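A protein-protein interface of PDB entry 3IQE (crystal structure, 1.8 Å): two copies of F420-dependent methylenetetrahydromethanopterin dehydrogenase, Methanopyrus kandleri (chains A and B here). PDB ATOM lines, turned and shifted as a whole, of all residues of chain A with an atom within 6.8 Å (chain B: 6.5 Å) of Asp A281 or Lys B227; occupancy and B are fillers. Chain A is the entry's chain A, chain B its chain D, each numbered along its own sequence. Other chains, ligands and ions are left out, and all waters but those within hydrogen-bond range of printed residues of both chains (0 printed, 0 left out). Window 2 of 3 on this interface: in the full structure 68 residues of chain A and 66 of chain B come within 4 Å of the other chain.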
ATOM      1  N   LEU A 273      28.264  14.477   7.361  1.00  0.00           N
ATOM      2  CA  LEU A 273      27.123  13.730   7.848  1.00  0.00           C
ATOM      3  C   LEU A 273      26.114  13.546   6.726  1.00  0.00           C
ATOM      4  O   LEU A 273      26.267  14.086   5.612  1.00  0.00           O
ATOM      5  CB  LEU A 273      26.484  14.469   9.001  1.00  0.00           C
ATOM      6  CG  LEU A 273      27.437  14.894  10.119  1.00  0.00           C
ATOM      7  CD1 LEU A 273      26.689  15.532  11.251  1.00  0.00           C
ATOM      8  CD2 LEU A 273      28.181  13.692  10.600  1.00  0.00           C
ATOM      9  N   SER A 274      25.062  12.798   7.008  1.00  0.00           N
ATOM     10  CA  SER A 274      24.009  12.619   6.015  1.00  0.00           C
ATOM     11  C   SER A 274      22.638  12.471   6.623  1.00  0.00           C
ATOM     12  O   SER A 274      22.496  11.979   7.768  1.00  0.00           O
ATOM     13  CB  SER A 274      24.281  11.374   5.190  1.00  0.00           C
ATOM     14  OG  SER A 274      23.741  11.576   3.907  1.00  0.00           O
ATOM     15  N   LYS A 275      21.632  12.874   5.835  1.00  0.00           N
ATOM     16  CA  LYS A 275      20.248  12.650   6.197  1.00  0.00           C
ATOM     17  C   LYS A 275      19.288  12.861   4.995  1.00  0.00           C
ATOM     18  O   LYS A 275      19.604  13.574   4.030  1.00  0.00           O
ATOM     19  CB  LYS A 275      19.895  13.567   7.389  1.00  0.00           C
ATOM     20  CG  LYS A 275      19.962  15.047   7.018  1.00  0.00           C
ATOM     21  CD  LYS A 275      19.502  15.961   8.133  1.00  0.00           C
ATOM     22  CE  LYS A 275      18.007  16.199   8.041  1.00  0.00           C
ATOM     23  NZ  LYS A 275      17.539  16.842   9.289  1.00  0.00           N
ATOM     24  N   LYS A 277      15.295  12.513   5.815  1.00  0.00           N
ATOM     25  CA  LYS A 277      14.045  13.012   6.380  1.00  0.00           C
ATOM     26  C   LYS A 277      14.243  14.307   7.176  1.00  0.00           C
ATOM     27  O   LYS A 277      15.224  14.465   7.894  1.00  0.00           O
ATOM     28  CB  LYS A 277      13.383  11.945   7.248  1.00  0.00           C
ATOM     29  CG  LYS A 277      13.054  10.673   6.465  1.00  0.00           C
ATOM     30  CD  LYS A 277      11.702  10.076   6.896  1.00  0.00           C
ATOM     31  CE  LYS A 277      11.073   9.293   5.748  1.00  0.00           C
ATOM     32  NZ  LYS A 277      10.916  10.146   4.499  1.00  0.00           N
ATOM     33  N   PHE A 278      13.305  15.233   7.041  1.00  0.00           N
ATOM     34  CA  PHE A 278      13.462  16.572   7.611  1.00  0.00           C
ATOM     35  C   PHE A 278      13.828  16.573   9.105  1.00  0.00           C
ATOM     36  O   PHE A 278      14.654  17.359   9.530  1.00  0.00           O
ATOM     37  CB  PHE A 278      12.167  17.370   7.390  1.00  0.00           C
ATOM     38  CG  PHE A 278      12.231  18.790   7.877  1.00  0.00           C
ATOM     39  CD1 PHE A 278      11.660  19.136   9.105  1.00  0.00           C
ATOM     40  CD2 PHE A 278      12.857  19.774   7.134  1.00  0.00           C
ATOM     41  CE1 PHE A 278      11.698  20.437   9.555  1.00  0.00           C
ATOM     42  CE2 PHE A 278      12.915  21.084   7.601  1.00  0.00           C
ATOM     43  CZ  PHE A 278      12.333  21.408   8.818  1.00  0.00           C
ATOM     44  N   MET A 279      13.188  15.723   9.912  1.00  0.00           N
ATOM     45  CA  MET A 279      13.429  15.724  11.356  1.00  0.00           C
ATOM     46  C   MET A 279      14.492  14.720  11.807  1.00  0.00           C
ATOM     47  O   MET A 279      14.695  14.546  13.003  1.00  0.00           O
ATOM     48  CB  MET A 279      12.152  15.418  12.164  1.00  0.00           C
ATOM     49  CG  MET A 279      10.936  16.339  11.964  1.00  0.00           C
ATOM     50  SD  MET A 279      11.237  18.113  12.176  1.00  0.00           S
ATOM     51  CE  MET A 279      12.374  18.148  13.572  1.00  0.00           C
ATOM     52  N   GLU A 280      15.146  14.012  10.897  1.00  0.00           N
ATOM     53  CA  GLU A 280      16.205  13.113  11.357  1.00  0.00           C
ATOM     54  C   GLU A 280      17.512  13.902  11.554  1.00  0.00           C
ATOM     55  O   GLU A 280      17.836  14.816  10.796  1.00  0.00           O
ATOM     56  CB  GLU A 280      16.372  11.898  10.426  1.00  0.00           C
ATOM     57  CG  GLU A 280      17.343  12.087   9.273  1.00  0.00           C
ATOM     58  CD  GLU A 280      17.389  10.912   8.281  1.00  0.00           C
ATOM     59  OE1 GLU A 280      16.640  10.934   7.283  1.00  0.00           O
ATOM     60  OE2 GLU A 280      18.216   9.986   8.460  1.00  0.00           O
ATOM     61  N   ASP A 281      18.245  13.560  12.605  1.00  0.00           N
ATOM     62  CA  ASP A 281      19.547  14.154  12.849  1.00  0.00           C
ATOM     63  C   ASP A 281      20.506  13.665  11.784  1.00  0.00           C
ATOM     64  O   ASP A 281      20.515  12.474  11.462  1.00  0.00           O
ATOM     65  CB  ASP A 281      20.073  13.719  14.215  1.00  0.00           C
ATOM     66  CG  ASP A 281      19.235  14.266  15.384  1.00  0.00           C
ATOM     67  OD1 ASP A 281      18.981  13.477  16.315  1.00  0.00           O
ATOM     68  OD2 ASP A 281      18.822  15.457  15.385  1.00  0.00           O
ATOM     69  N   PRO A 282      21.340  14.568  11.243  1.00  0.00           N
ATOM     70  CA  PRO A 282      22.361  14.091  10.310  1.00  0.00           C
ATOM     71  C   PRO A 282      23.341  13.175  11.015  1.00  0.00           C
ATOM     72  O   PRO A 282      23.650  13.402  12.191  1.00  0.00           O
ATOM     73  CB  PRO A 282      23.053  15.378   9.852  1.00  0.00           C
ATOM     74  CG  PRO A 282      22.819  16.349  10.952  1.00  0.00           C
ATOM     75  CD  PRO A 282      21.451  16.014  11.488  1.00  0.00           C
ATOM     76  N   GLU A 283      23.820  12.143  10.328  1.00  0.00           N
ATOM     77  CA  GLU A 283      24.724  11.181  10.962  1.00  0.00           C
ATOM     78  C   GLU A 283      25.806  10.651  10.024  1.00  0.00           C
ATOM     79  O   GLU A 283      26.741   9.989  10.478  1.00  0.00           O
ATOM     80  CB  GLU A 283      23.914  10.016  11.507  1.00  0.00           C
ATOM     81  CG  GLU A 283      22.895  10.448  12.558  1.00  0.00           C
ATOM     82  CD  GLU A 283      21.908   9.361  12.900  1.00  0.00           C
ATOM     83  OE1 GLU A 283      22.055   8.728  13.983  1.00  0.00           O
ATOM     84  OE2 GLU A 283      20.992   9.143  12.086  1.00  0.00           O
ATOM     85  OXT GLU A 283      25.792  10.857   8.811  1.00  0.00           O
ATOM     86  N   GLU B 130      21.148  20.608  11.412  1.00  0.00           N
ATOM     87  CA  GLU B 130      20.104  19.646  10.993  1.00  0.00           C
ATOM     88  C   GLU B 130      19.452  20.030   9.658  1.00  0.00           C
ATOM     89  O   GLU B 130      18.882  19.189   8.969  1.00  0.00           O
ATOM     90  CB  GLU B 130      19.044  19.521  12.089  1.00  0.00           C
ATOM     91  CG  GLU B 130      19.552  18.963  13.423  1.00  0.00           C
ATOM     92  CD  GLU B 130      19.892  20.054  14.465  1.00  0.00           C
ATOM     93  OE1 GLU B 130      19.881  19.746  15.680  1.00  0.00           O
ATOM     94  OE2 GLU B 130      20.166  21.212  14.064  1.00  0.00           O
ATOM     95  N   GLU B 224      15.372  29.800  20.415  1.00  0.00           N
ATOM     96  CA  GLU B 224      14.793  28.472  20.576  1.00  0.00           C
ATOM     97  C   GLU B 224      15.867  27.381  20.760  1.00  0.00           C
ATOM     98  O   GLU B 224      16.754  27.238  19.934  1.00  0.00           O
ATOM     99  CB  GLU B 224      13.892  28.150  19.385  1.00  0.00           C
ATOM    100  CG  GLU B 224      13.229  26.799  19.434  1.00  0.00           C
ATOM    101  CD  GLU B 224      12.319  26.630  20.653  1.00  0.00           C
ATOM    102  OE1 GLU B 224      12.612  25.759  21.509  1.00  0.00           O
ATOM    103  OE2 GLU B 224      11.323  27.381  20.748  1.00  0.00           O
ATOM    104  N   GLN B 225      15.767  26.598  21.829  1.00  0.00           N
ATOM    105  CA  GLN B 225      16.778  25.561  22.113  1.00  0.00           C
ATOM    106  C   GLN B 225      16.347  24.122  21.794  1.00  0.00           C
ATOM    107  O   GLN B 225      17.168  23.223  21.840  1.00  0.00           O
ATOM    108  CB  GLN B 225      17.239  25.654  23.578  1.00  0.00           C
ATOM    109  CG  GLN B 225      17.888  26.955  23.894  1.00  0.00           C
ATOM    110  CD  GLN B 225      19.103  27.181  23.041  1.00  0.00           C
ATOM    111  OE1 GLN B 225      20.081  26.439  23.149  1.00  0.00           O
ATOM    112  NE2 GLN B 225      19.057  28.196  22.175  1.00  0.00           N
ATOM    113  N   ASP B 226      15.072  23.925  21.460  1.00  0.00           N
ATOM    114  CA  ASP B 226      14.482  22.610  21.238  1.00  0.00           C
ATOM    115  C   ASP B 226      14.444  22.338  19.716  1.00  0.00           C
ATOM    116  O   ASP B 226      13.751  23.041  19.002  1.00  0.00           O
ATOM    117  CB  ASP B 226      13.059  22.636  21.796  1.00  0.00           C
ATOM    118  CG  ASP B 226      12.367  21.305  21.702  1.00  0.00           C
ATOM    119  OD1 ASP B 226      11.231  21.215  22.246  1.00  0.00           O
ATOM    120  OD2 ASP B 226      12.921  20.356  21.075  1.00  0.00           O
ATOM    121  N   LYS B 227      15.204  21.351  19.242  1.00  0.00           N
ATOM    122  CA  LYS B 227      15.388  21.106  17.803  1.00  0.00           C
ATOM    123  C   LYS B 227      14.085  20.774  17.053  1.00  0.00           C
ATOM    124  O   LYS B 227      13.962  21.009  15.833  1.00  0.00           O
ATOM    125  CB  LYS B 227      16.384  19.970  17.594  1.00  0.00           C
ATOM    126  CG  LYS B 227      15.955  18.657  18.212  1.00  0.00           C
ATOM    127  CD  LYS B 227      16.759  17.448  17.717  1.00  0.00           C
ATOM    128  CE  LYS B 227      18.077  17.289  18.431  1.00  0.00           C
ATOM    129  NZ  LYS B 227      18.461  15.841  18.529  1.00  0.00           N
ATOM    130  N   GLU B 228      13.130  20.188  17.774  1.00  0.00           N
ATOM    131  CA  GLU B 228      11.808  19.901  17.249  1.00  0.00           C
ATOM    132  C   GLU B 228      11.086  21.187  16.885  1.00  0.00           C
ATOM    133  O   GLU B 228      10.123  21.165  16.125  1.00  0.00           O
ATOM    134  CB  GLU B 228      10.942  19.169  18.276  1.00  0.00           C
ATOM    135  CG  GLU B 228      11.027  17.650  18.246  1.00  0.00           C
ATOM    136  CD  GLU B 228       9.754  16.983  18.784  1.00  0.00           C
ATOM    137  OE1 GLU B 228       9.873  15.977  19.515  1.00  0.00           O
ATOM    138  OE2 GLU B 228       8.629  17.466  18.475  1.00  0.00           O
ATOM    139  N   ARG B 229      11.503  22.284  17.511  1.00  0.00           N
ATOM    140  CA  ARG B 229      10.961  23.591  17.190  1.00  0.00           C
ATOM    141  C   ARG B 229      11.954  24.343  16.282  1.00  0.00           C
ATOM    142  O   ARG B 229      11.583  24.920  15.244  1.00  0.00           O
ATOM    143  CB  ARG B 229      10.732  24.396  18.469  1.00  0.00           C
ATOM    144  CG  ARG B 229       9.567  23.857  19.367  1.00  0.00           C
ATOM    145  CD  ARG B 229       9.427  24.685  20.628  1.00  0.00           C
ATOM    146  NE  ARG B 229       8.906  26.024  20.377  1.00  0.00           N
ATOM    147  CZ  ARG B 229       7.616  26.327  20.322  1.00  0.00           C
ATOM    148  NH1 ARG B 229       7.238  27.567  20.096  1.00  0.00           N
ATOM    149  NH2 ARG B 229       6.706  25.395  20.460  1.00  0.00           N
ATOM    150  N   TYR B 230      13.227  24.330  16.618  1.00  0.00           N
ATOM    151  CA  TYR B 230      14.146  25.195  15.852  1.00  0.00           C
ATOM    152  C   TYR B 230      14.417  24.741  14.402  1.00  0.00           C
ATOM    153  O   TYR B 230      14.704  25.569  13.547  1.00  0.00           O
ATOM    154  CB  TYR B 230      15.449  25.529  16.621  1.00  0.00           C
ATOM    155  CG  TYR B 230      16.479  24.454  16.782  1.00  0.00           C
ATOM    156  CD1 TYR B 230      16.941  24.123  18.059  1.00  0.00           C
ATOM    157  CD2 TYR B 230      17.068  23.830  15.697  1.00  0.00           C
ATOM    158  CE1 TYR B 230      17.895  23.169  18.250  1.00  0.00           C
ATOM    159  CE2 TYR B 230      18.062  22.876  15.881  1.00  0.00           C
ATOM    160  CZ  TYR B 230      18.451  22.540  17.187  1.00  0.00           C
ATOM    161  OH  TYR B 230      19.460  21.638  17.438  1.00  0.00           O
ATOM    162  N   VAL B 231      14.271  23.456  14.094  1.00  0.00           N
ATOM    163  CA  VAL B 231      14.543  23.038  12.729  1.00  0.00           C
ATOM    164  C   VAL B 231      13.422  23.549  11.796  1.00  0.00           C
ATOM    165  O   VAL B 231      13.694  24.259  10.819  1.00  0.00           O
ATOM    166  CB  VAL B 231      14.852  21.527  12.586  1.00  0.00           C
ATOM    167  CG1 VAL B 231      15.170  21.178  11.126  1.00  0.00           C
ATOM    168  CG2 VAL B 231      16.016  21.162  13.454  1.00  0.00           C
ATOM    169  N   PRO B 232      12.165  23.314  12.152  1.00  0.00           N
ATOM    170  CA  PRO B 232      11.116  23.937  11.324  1.00  0.00           C
ATOM    171  C   PRO B 232      11.178  25.442  11.286  1.00  0.00           C
ATOM    172  O   PRO B 232      10.912  26.031  10.255  1.00  0.00           O
ATOM    173  CB  PRO B 232       9.845  23.528  12.000  1.00  0.00           C
ATOM    174  CG  PRO B 232      10.197  22.531  13.011  1.00  0.00           C
ATOM    175  CD  PRO B 232      11.621  22.326  13.096  1.00  0.00           C
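Of the 10 printed residues of chain B, 4 touch a printed residue of chain A.
Hydrophobic or aromatic side chains of chain B that line the printed part of chain A: Val B231.
Printed residues of chain A that touch a printed residue of chain B: Lys A275, Phe A278, Met A279, Asp A281 and Pro A282.
Hydrophobic or aromatic side chains of chain A within 4 Å of the printed part of chain B: Phe A278, Met A279 and Pro A282.
The side-chain amino group (NZ) of Lys A275 lies within hydrogen-bond range of the backbone carbonyl oxygen (O) of Phe A278, at 2.9 Å.
NZ of Lys A275 lies within hydrogen-bond range of O of Glu A280.
OE1 of Glu B130 is in hydrogen-bond range of OH of Tyr B230.
The side-chain amino group (NZ) of Lys A275 lies within hydrogen-bond range of the backbone carbonyl oxygen (O) of Glu B130 (2.7 Å).
NZ of Lys B227 is in salt-bridge range of OD2 of Asp A281, 3.2 Å away.
No position is printed for both chains.
Of the 6 pairs that touch across the chains among the printed residues, none has its exchanged pair printed and touching as well.
Printed residues of chain B within 4 Å of Asp A281: Lys B227.
Of the printed residues of chain A, Lys B227 touches Met A279 (3.98 Å) and Asp A281 (3.2 Å).
Of the printed residues of chain A, Pro B232 touches Phe A278.
Printed residues of chain A within 4 Å of Val B231: Phe A278 (3.7 Å).
Of the printed residues of chain B, Lys A275 touches Glu B130.
Printed residues of chain B within 4 Å of Met A279: Lys B227 (3.98 Å).
Gln B225 touches none of the printed residues of chain A.
Glu B228 touches none of the printed residues of chain A.
The nearest printed residue of chain B that does not touch Met A279 is Glu B228 (4.1 Å).
Among the printed residues, pairs that only touch across the chains: Phe A278 with Val B231, Phe A278 with Pro B232, Met A279 with Lys B227 and Pro A282 with Glu B130.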
